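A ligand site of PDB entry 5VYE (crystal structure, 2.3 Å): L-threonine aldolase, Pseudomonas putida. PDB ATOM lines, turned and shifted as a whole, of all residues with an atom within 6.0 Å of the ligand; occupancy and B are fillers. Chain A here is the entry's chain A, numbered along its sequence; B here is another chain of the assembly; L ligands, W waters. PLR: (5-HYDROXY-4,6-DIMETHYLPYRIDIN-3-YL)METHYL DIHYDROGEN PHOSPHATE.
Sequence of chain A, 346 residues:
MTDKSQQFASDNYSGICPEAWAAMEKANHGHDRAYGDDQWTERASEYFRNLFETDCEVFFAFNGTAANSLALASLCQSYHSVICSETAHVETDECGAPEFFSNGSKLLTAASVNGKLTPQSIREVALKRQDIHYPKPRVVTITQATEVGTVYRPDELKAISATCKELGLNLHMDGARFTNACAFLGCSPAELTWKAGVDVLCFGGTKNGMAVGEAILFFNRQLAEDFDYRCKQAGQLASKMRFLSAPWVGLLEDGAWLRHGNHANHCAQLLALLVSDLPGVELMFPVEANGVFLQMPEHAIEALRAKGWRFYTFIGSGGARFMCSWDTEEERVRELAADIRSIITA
The backbone NH (N) of Tyr 35 of chain B lies within hydrogen-bond range of the backbone carbonyl oxygen (O) of Ser 239 of chain B (3.4 Å). The backbone NH of Thr 65 sits at hydrogen-bond distance from the side-chain amide oxygen of Asn 63, 3.2 Å away. The side-chain amide oxygen of Asn 68 sits close to the backbone carbonyl oxygen of Gly 64. N of Ala 176 lies within hydrogen-bond range of OD1 of Asp 174 (3.1 Å). The backbone NH (N) of Ala 66 is in hydrogen-bond range of the side-chain amide oxygen (OD1) of Asn 63. O of Arg 177 lies within hydrogen-bond range of N of Ala 145 (3.0 Å). The side-chain carboxylate (OD2) of Asp 174 sits close to the side-chain amide oxygen (OD1) of Asn 68. The side-chain carboxylate of Glu 147 is in hydrogen-bond range of the backbone NH of His 89 (2.8 Å).
The backbone NH (N) of Thr 65 sits at hydrogen-bond distance from an oxygen (O2P) of the ligand (2.9 Å). A nitrogen (N1) of the ligand sits at hydrogen-bond distance from the side-chain carboxylate of Asp 174 (2.5 Å). The side-chain amino group (NZ) of Lys 207 is in hydrogen-bond range of an oxygen (O3) of the ligand (2.5 Å). The backbone NH (N) of Gly 64 sits at hydrogen-bond distance from an oxygen (O1P) of the ligand (3.3 Å). OG1 of Thr 65 lies within hydrogen-bond range of O2P of the ligand, 2.9 Å away. O3P of the ligand is in hydrogen-bond range of OH of Tyr 35 of chain B. A ring nitrogen (ND1) of His 89 sits close to a nitrogen (N1) of the ligand.
Water W1 lies within hydrogen-bond range of OE2 of Glu 214 and O4P of the ligand. Water W2 lies within hydrogen-bond range of NH1 of Arg 177 (2.9 Å), O of Ala 145 (3.0 Å) and O of Thr 146 (3.5 Å). Water W3 lies within hydrogen-bond range of OD1 of Asp 174 and OE2 of Glu 214. Water W4 lies within hydrogen-bond range of OG1 of Thr 65 (3.2 Å), O2P of the ligand (3.3 Å) and NZ of Lys 232 of chain B (3.5 Å).
Residues that only touch the ligand: Asn 68 (3.5 Å), Asn 63 (3.5 Å), Ala 176 (3.6 Å), Arg 177 (3.6 Å), Thr 143 (3.7 Å) and Glu 94 (3.9 Å). Hydrophobic or aromatic side chains that line the ligand: His 89, Ala 176 and Tyr 35 of chain B. Within 4 Å of the ligand: Asn 63, Gly 64, Thr 65, Asn 68, His 89, Glu 94, Thr 143, Asp 174, Ala 176, Arg 177, Lys 207 and Tyr 35 of chain B.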
ATOM      1  N   ASN A  12      37.895 -10.023 -15.667  1.00  0.00           N
ATOM      2  CA  ASN A  12      37.348  -9.943 -17.015  1.00  0.00           C
ATOM      3  C   ASN A  12      38.417  -9.793 -18.074  1.00  0.00           C
ATOM      4  O   ASN A  12      38.089  -9.856 -19.255  1.00  0.00           O
ATOM      5  CB  ASN A  12      36.385  -8.762 -17.145  1.00  0.00           C
ATOM      6  CG  ASN A  12      35.048  -9.010 -16.516  1.00  0.00           C
ATOM      7  OD1 ASN A  12      34.502 -10.112 -16.588  1.00  0.00           O
ATOM      8  ND2 ASN A  12      34.483  -7.965 -15.917  1.00  0.00           N
ATOM      9  N   PHE A  62      24.445 -14.314 -23.620  1.00  0.00           N
ATOM     10  CA  PHE A  62      25.752 -13.882 -24.106  1.00  0.00           C
ATOM     11  C   PHE A  62      26.605 -13.295 -22.976  1.00  0.00           C
ATOM     12  O   PHE A  62      27.837 -13.439 -23.003  1.00  0.00           O
ATOM     13  CB  PHE A  62      25.606 -12.845 -25.241  1.00  0.00           C
ATOM     14  CG  PHE A  62      25.112 -13.416 -26.550  1.00  0.00           C
ATOM     15  CD1 PHE A  62      25.844 -14.381 -27.249  1.00  0.00           C
ATOM     16  CD2 PHE A  62      23.906 -12.985 -27.084  1.00  0.00           C
ATOM     17  CE1 PHE A  62      25.376 -14.888 -28.484  1.00  0.00           C
ATOM     18  CE2 PHE A  62      23.440 -13.482 -28.273  1.00  0.00           C
ATOM     19  CZ  PHE A  62      24.172 -14.427 -28.985  1.00  0.00           C
ATOM     20  N   ASN A  63      26.029 -12.613 -21.983  1.00  0.00           N
ATOM     21  CA  ASN A  63      26.845 -12.016 -20.932  1.00  0.00           C
ATOM     22  C   ASN A  63      26.004 -11.890 -19.673  1.00  0.00           C
ATOM     23  O   ASN A  63      24.809 -12.187 -19.673  1.00  0.00           O
ATOM     24  CB  ASN A  63      27.408 -10.652 -21.368  1.00  0.00           C
ATOM     25  CG  ASN A  63      26.319  -9.524 -21.471  1.00  0.00           C
ATOM     26  OD1 ASN A  63      25.222  -9.621 -20.952  1.00  0.00           O
ATOM     27  ND2 ASN A  63      26.667  -8.468 -22.128  1.00  0.00           N
ATOM     28  N   GLY A  64      26.620 -11.390 -18.593  1.00  0.00           N
ATOM     29  CA  GLY A  64      25.971 -11.415 -17.290  1.00  0.00           C
ATOM     30  C   GLY A  64      25.005 -10.284 -17.103  1.00  0.00           C
ATOM     31  O   GLY A  64      24.022 -10.428 -16.356  1.00  0.00           O
ATOM     32  N   THR A  65      25.249  -9.149 -17.751  1.00  0.00           N
ATOM     33  CA  THR A  65      24.298  -8.056 -17.711  1.00  0.00           C
ATOM     34  C   THR A  65      22.949  -8.520 -18.237  1.00  0.00           C
ATOM     35  O   THR A  65      21.912  -8.341 -17.585  1.00  0.00           O
ATOM     36  CB  THR A  65      24.837  -6.855 -18.500  1.00  0.00           C
ATOM     37  OG1 THR A  65      25.968  -6.314 -17.818  1.00  0.00           O
ATOM     38  CG2 THR A  65      23.768  -5.697 -18.620  1.00  0.00           C
ATOM     39  N   ALA A  66      22.962  -9.146 -19.416  1.00  0.00           N
ATOM     40  CA  ALA A  66      21.713  -9.673 -19.976  1.00  0.00           C
ATOM     41  C   ALA A  66      21.183 -10.839 -19.160  1.00  0.00           C
ATOM     42  O   ALA A  66      19.967 -10.948 -18.935  1.00  0.00           O
ATOM     43  CB  ALA A  66      21.941 -10.092 -21.410  1.00  0.00           C
ATOM     44  N   ASN A  68      21.388 -11.523 -15.905  1.00  0.00           N
ATOM     45  CA  ASN A  68      20.668 -11.064 -14.726  1.00  0.00           C
ATOM     46  C   ASN A  68      19.423 -10.273 -15.106  1.00  0.00           C
ATOM     47  O   ASN A  68      18.406 -10.312 -14.409  1.00  0.00           O
ATOM     48  CB  ASN A  68      21.544 -10.127 -13.882  1.00  0.00           C
ATOM     49  CG  ASN A  68      22.707 -10.810 -13.191  1.00  0.00           C
ATOM     50  OD1 ASN A  68      23.706 -10.154 -12.934  1.00  0.00           O
ATOM     51  ND2 ASN A  68      22.592 -12.040 -12.845  1.00  0.00           N
ATOM     52  N   HIS A  89      25.762  -5.269  -8.714  1.00  0.00           N
ATOM     53  CA  HIS A  89      26.079  -5.011 -10.102  1.00  0.00           C
ATOM     54  C   HIS A  89      24.854  -4.500 -10.875  1.00  0.00           C
ATOM     55  O   HIS A  89      24.963  -3.570 -11.679  1.00  0.00           O
ATOM     56  CB  HIS A  89      26.669  -6.291 -10.725  1.00  0.00           C
ATOM     57  CG  HIS A  89      27.415  -6.060 -11.997  1.00  0.00           C
ATOM     58  ND1 HIS A  89      26.847  -6.239 -13.244  1.00  0.00           N
ATOM     59  CD2 HIS A  89      28.690  -5.674 -12.211  1.00  0.00           C
ATOM     60  CE1 HIS A  89      27.749  -5.935 -14.177  1.00  0.00           C
ATOM     61  NE2 HIS A  89      28.874  -5.598 -13.570  1.00  0.00           N
ATOM     62  N   VAL A  90      23.681  -5.078 -10.629  1.00  0.00           N
ATOM     63  CA  VAL A  90      22.503  -4.662 -11.381  1.00  0.00           C
ATOM     64  C   VAL A  90      22.198  -3.229 -11.102  1.00  0.00           C
ATOM     65  O   VAL A  90      21.549  -2.579 -11.914  1.00  0.00           O
ATOM     66  CB  VAL A  90      21.255  -5.504 -11.078  1.00  0.00           C
ATOM     67  CG1 VAL A  90      21.398  -6.902 -11.716  1.00  0.00           C
ATOM     68  CG2 VAL A  90      21.043  -5.596  -9.552  1.00  0.00           C
ATOM     69  N   ASP A  93      26.375  -1.211 -12.317  1.00  0.00           N
ATOM     70  CA  ASP A  93      27.309  -1.548 -13.398  1.00  0.00           C
ATOM     71  C   ASP A  93      26.661  -1.959 -14.701  1.00  0.00           C
ATOM     72  O   ASP A  93      27.369  -2.459 -15.583  1.00  0.00           O
ATOM     73  CB  ASP A  93      28.256  -2.661 -12.931  1.00  0.00           C
ATOM     74  CG  ASP A  93      29.335  -2.142 -12.026  1.00  0.00           C
ATOM     75  OD1 ASP A  93      29.238  -0.965 -11.603  1.00  0.00           O
ATOM     76  OD2 ASP A  93      30.274  -2.900 -11.733  1.00  0.00           O
ATOM     77  N   GLU A  94      25.360  -1.725 -14.901  1.00  0.00           N
ATOM     78  CA  GLU A  94      24.674  -2.287 -16.064  1.00  0.00           C
ATOM     79  C   GLU A  94      23.970  -1.217 -16.908  1.00  0.00           C
ATOM     80  O   GLU A  94      23.113  -1.551 -17.729  1.00  0.00           O
ATOM     81  CB  GLU A  94      23.727  -3.396 -15.602  1.00  0.00           C
ATOM     82  CG  GLU A  94      24.524  -4.633 -15.170  1.00  0.00           C
ATOM     83  CD  GLU A  94      23.679  -5.856 -14.739  1.00  0.00           C
ATOM     84  OE1 GLU A  94      22.466  -5.943 -15.125  1.00  0.00           O
ATOM     85  OE2 GLU A  94      24.224  -6.750 -14.019  1.00  0.00           O
ATOM     86  N   THR A 143      24.272 -11.448  -4.755  1.00  0.00           N
ATOM     87  CA  THR A 143      25.470 -11.757  -5.536  1.00  0.00           C
ATOM     88  C   THR A 143      26.411 -12.696  -4.772  1.00  0.00           C
ATOM     89  O   THR A 143      26.691 -12.452  -3.613  1.00  0.00           O
ATOM     90  CB  THR A 143      26.195 -10.470  -5.866  1.00  0.00           C
ATOM     91  OG1 THR A 143      25.253  -9.512  -6.380  1.00  0.00           O
ATOM     92  CG2 THR A 143      27.221 -10.742  -6.873  1.00  0.00           C
ATOM     93  N   ALA A 145      30.004 -15.058  -5.533  1.00  0.00           N
ATOM     94  CA  ALA A 145      30.471 -14.148  -4.485  1.00  0.00           C
ATOM     95  C   ALA A 145      30.117 -12.681  -4.788  1.00  0.00           C
ATOM     96  O   ALA A 145      29.863 -12.318  -5.949  1.00  0.00           O
ATOM     97  CB  ALA A 145      32.002 -14.290  -4.289  1.00  0.00           C
ATOM     98  N   THR A 146      30.140 -11.853  -3.752  1.00  0.00           N
ATOM     99  CA  THR A 146      29.718 -10.464  -3.853  1.00  0.00           C
ATOM    100  C   THR A 146      30.753  -9.622  -4.569  1.00  0.00           C
ATOM    101  O   THR A 146      31.877 -10.047  -4.873  1.00  0.00           O
ATOM    102  CB  THR A 146      29.491  -9.846  -2.477  1.00  0.00           C
ATOM    103  OG1 THR A 146      30.778  -9.507  -1.932  1.00  0.00           O
ATOM    104  CG2 THR A 146      28.738 -10.784  -1.550  1.00  0.00           C
ATOM    105  N   GLU A 147      30.332  -8.368  -4.772  1.00  0.00           N
ATOM    106  CA  GLU A 147      31.082  -7.334  -5.479  1.00  0.00           C
ATOM    107  C   GLU A 147      32.284  -6.822  -4.684  1.00  0.00           C
ATOM    108  O   GLU A 147      33.083  -6.049  -5.220  1.00  0.00           O
ATOM    109  CB  GLU A 147      30.143  -6.165  -5.792  1.00  0.00           C
ATOM    110  CG  GLU A 147      28.976  -6.462  -6.788  1.00  0.00           C
ATOM    111  CD  GLU A 147      27.715  -7.012  -6.145  1.00  0.00           C
ATOM    112  OE1 GLU A 147      27.711  -7.316  -4.924  1.00  0.00           O
ATOM    113  OE2 GLU A 147      26.716  -7.144  -6.922  1.00  0.00           O
ATOM    114  N   ASP A 174      23.022 -13.773  -8.547  1.00  0.00           N
ATOM    115  CA  ASP A 174      24.007 -13.358  -9.525  1.00  0.00           C
ATOM    116  C   ASP A 174      25.300 -14.082  -9.203  1.00  0.00           C
ATOM    117  O   ASP A 174      26.023 -13.682  -8.293  1.00  0.00           O
ATOM    118  CB  ASP A 174      24.197 -11.863  -9.451  1.00  0.00           C
ATOM    119  CG  ASP A 174      25.259 -11.353 -10.394  1.00  0.00           C
ATOM    120  OD1 ASP A 174      25.916 -12.168 -11.103  1.00  0.00           O
ATOM    121  OD2 ASP A 174      25.398 -10.115 -10.459  1.00  0.00           O
ATOM    122  N   ALA A 176      28.037 -14.437 -10.989  1.00  0.00           N
ATOM    123  CA  ALA A 176      29.144 -14.048 -11.851  1.00  0.00           C
ATOM    124  C   ALA A 176      30.470 -14.647 -11.330  1.00  0.00           C
ATOM    125  O   ALA A 176      31.278 -15.176 -12.102  1.00  0.00           O
ATOM    126  CB  ALA A 176      29.193 -12.533 -11.918  1.00  0.00           C
ATOM    127  N   ARG A 177      30.653 -14.644 -10.025  1.00  0.00           N
ATOM    128  CA  ARG A 177      31.804 -15.268  -9.356  1.00  0.00           C
ATOM    129  C   ARG A 177      31.354 -16.417  -8.476  1.00  0.00           C
ATOM    130  O   ARG A 177      31.831 -16.594  -7.354  1.00  0.00           O
ATOM    131  CB  ARG A 177      32.571 -14.225  -8.552  1.00  0.00           C
ATOM    132  CG  ARG A 177      33.139 -13.129  -9.470  1.00  0.00           C
ATOM    133  CD  ARG A 177      34.192 -12.278  -8.797  1.00  0.00           C
ATOM    134  NE  ARG A 177      34.873 -11.370  -9.723  1.00  0.00           N
ATOM    135  CZ  ARG A 177      34.406 -10.171 -10.066  1.00  0.00           C
ATOM    136  NH1 ARG A 177      33.248  -9.703  -9.593  1.00  0.00           N
ATOM    137  NH2 ARG A 177      35.089  -9.433 -10.917  1.00  0.00           N
ATOM    138  N   THR A 206      32.308 -16.452 -18.366  1.00  0.00           N
ATOM    139  CA  THR A 206      33.303 -15.545 -18.933  1.00  0.00           C
ATOM    140  C   THR A 206      34.407 -15.221 -17.921  1.00  0.00           C
ATOM    141  O   THR A 206      35.586 -15.262 -18.267  1.00  0.00           O
ATOM    142  CB  THR A 206      32.629 -14.279 -19.455  1.00  0.00           C
ATOM    143  OG1 THR A 206      31.751 -14.613 -20.528  1.00  0.00           O
ATOM    144  CG2 THR A 206      33.623 -13.328 -20.013  1.00  0.00           C
ATOM    145  N   LYS A 207      34.051 -14.894 -16.678  1.00  0.00           N
ATOM    146  CA  LYS A 207      35.094 -14.469 -15.747  1.00  0.00           C
ATOM    147  C   LYS A 207      36.065 -15.584 -15.400  1.00  0.00           C
ATOM    148  O   LYS A 207      37.229 -15.308 -15.047  1.00  0.00           O
ATOM    149  CB  LYS A 207      34.498 -13.935 -14.468  1.00  0.00           C
ATOM    150  CG  LYS A 207      34.440 -12.468 -14.466  1.00  0.00           C
ATOM    151  CD  LYS A 207      33.500 -11.937 -13.421  1.00  0.00           C
ATOM    152  CE  LYS A 207      33.035 -10.540 -13.822  1.00  0.00           C
ATOM    153  NZ  LYS A 207      32.262  -9.937 -12.726  1.00  0.00           N
ATOM    154  N   GLU A 214      27.066 -16.851 -20.454  1.00  0.00           N
ATOM    155  CA  GLU A 214      26.690 -17.149 -19.080  1.00  0.00           C
ATOM    156  C   GLU A 214      25.649 -18.256 -19.138  1.00  0.00           C
ATOM    157  O   GLU A 214      24.889 -18.348 -20.105  1.00  0.00           O
ATOM    158  CB  GLU A 214      26.032 -15.963 -18.289  1.00  0.00           C
ATOM    159  CG  GLU A 214      26.956 -14.907 -17.786  1.00  0.00           C
ATOM    160  CD  GLU A 214      26.769 -14.523 -16.328  1.00  0.00           C
ATOM    161  OE1 GLU A 214      25.804 -14.919 -15.645  1.00  0.00           O
ATOM    162  OE2 GLU A 214      27.633 -13.759 -15.852  1.00  0.00           O
ATOM    163  N   TYR B  35      35.498  -4.335 -23.081  1.00  0.00           N
ATOM    164  CA  TYR B  35      34.374  -3.512 -23.534  1.00  0.00           C
ATOM    165  C   TYR B  35      34.720  -2.625 -24.737  1.00  0.00           C
ATOM    166  O   TYR B  35      34.022  -1.638 -25.006  1.00  0.00           O
ATOM    167  CB  TYR B  35      33.826  -2.641 -22.388  1.00  0.00           C
ATOM    168  CG  TYR B  35      33.365  -3.419 -21.155  1.00  0.00           C
ATOM    169  CD1 TYR B  35      32.286  -4.310 -21.223  1.00  0.00           C
ATOM    170  CD2 TYR B  35      33.996  -3.268 -19.924  1.00  0.00           C
ATOM    171  CE1 TYR B  35      31.864  -5.029 -20.101  1.00  0.00           C
ATOM    172  CE2 TYR B  35      33.570  -3.978 -18.796  1.00  0.00           C
ATOM    173  CZ  TYR B  35      32.508  -4.867 -18.898  1.00  0.00           C
ATOM    174  OH  TYR B  35      32.076  -5.577 -17.795  1.00  0.00           O
ATOM    175  N   LYS B 232      25.150  -1.131 -24.283  1.00  0.00           N
ATOM    176  CA  LYS B 232      25.437  -1.644 -22.942  1.00  0.00           C
ATOM    177  C   LYS B 232      24.140  -1.917 -22.209  1.00  0.00           C
ATOM    178  O   LYS B 232      23.959  -3.002 -21.640  1.00  0.00           O
ATOM    179  CB  LYS B 232      26.295  -0.686 -22.165  1.00  0.00           C
ATOM    180  CG  LYS B 232      26.434  -0.917 -20.652  1.00  0.00           C
ATOM    181  CD  LYS B 232      27.660  -1.655 -20.271  1.00  0.00           C
ATOM    182  CE  LYS B 232      27.978  -1.432 -18.776  1.00  0.00           C
ATOM    183  NZ  LYS B 232      28.582  -2.644 -18.165  1.00  0.00           N
ATOM    184  N   LEU B 237      27.059  -5.713 -24.879  1.00  0.00           N
ATOM    185  CA  LEU B 237      28.456  -5.286 -24.782  1.00  0.00           C
ATOM    186  C   LEU B 237      29.308  -6.435 -24.275  1.00  0.00           C
ATOM    187  O   LEU B 237      29.118  -6.917 -23.147  1.00  0.00           O
ATOM    188  CB  LEU B 237      28.621  -4.120 -23.818  1.00  0.00           C
ATOM    189  CG  LEU B 237      29.906  -3.344 -23.991  1.00  0.00           C
ATOM    190  CD1 LEU B 237      29.721  -2.435 -25.226  1.00  0.00           C
ATOM    191  CD2 LEU B 237      30.159  -2.550 -22.735  1.00  0.00           C
ATOM    192  N   SER B 239      32.297  -8.255 -22.643  1.00  0.00           N
ATOM    193  CA  SER B 239      33.396  -8.077 -21.697  1.00  0.00           C
ATOM    194  C   SER B 239      34.746  -8.374 -22.361  1.00  0.00           C
ATOM    195  O   SER B 239      35.712  -7.630 -22.188  1.00  0.00           O
ATOM    196  CB  SER B 239      33.181  -9.013 -20.514  1.00  0.00           C
ATOM    197  OG  SER B 239      34.146  -8.693 -19.542  1.00  0.00           O
HETATM  198  N1  PLR L   1      27.149  -9.423 -12.095  1.00  0.00           N
HETATM  199  C2  PLR L   1      28.351  -9.071 -11.483  1.00  0.00           C
HETATM  200  C2A PLR L   1      28.565  -9.136  -9.950  1.00  0.00           C
HETATM  201  C3  PLR L   1      29.452  -8.635 -12.284  1.00  0.00           C
HETATM  202  O3  PLR L   1      30.676  -8.280 -11.663  1.00  0.00           O
HETATM  203  C4  PLR L   1      29.352  -8.541 -13.651  1.00  0.00           C
HETATM  204  C4A PLR L   1      30.580  -8.008 -14.488  1.00  0.00           C
HETATM  205  C5  PLR L   1      28.124  -8.893 -14.220  1.00  0.00           C
HETATM  206  C6  PLR L   1      27.026  -9.331 -13.453  1.00  0.00           C
HETATM  207  C5A PLR L   1      27.934  -8.751 -15.721  1.00  0.00           C
HETATM  208  O4P PLR L   1      29.006  -9.385 -16.399  1.00  0.00           O
HETATM  209  P   PLR L   1      29.156  -9.012 -18.035  1.00  0.00           P
HETATM  210  O1P PLR L   1      29.757 -10.383 -18.686  1.00  0.00           O
HETATM  211  O2P PLR L   1      27.919  -8.305 -18.653  1.00  0.00           O
HETATM  212  O3P PLR L   1      30.197  -7.841 -17.982  1.00  0.00           O
HETATM  213  O   HOH W   1      29.807 -12.335 -15.430  1.00  0.00           O
HETATM  214  O   HOH W   2      30.902 -10.558  -8.191  1.00  0.00           O
HETATM  215  O   HOH W   3      26.221 -12.536 -13.626  1.00  0.00           O
HETATM  216  O   HOH W   4      27.921  -5.350 -20.220  1.00  0.00           O
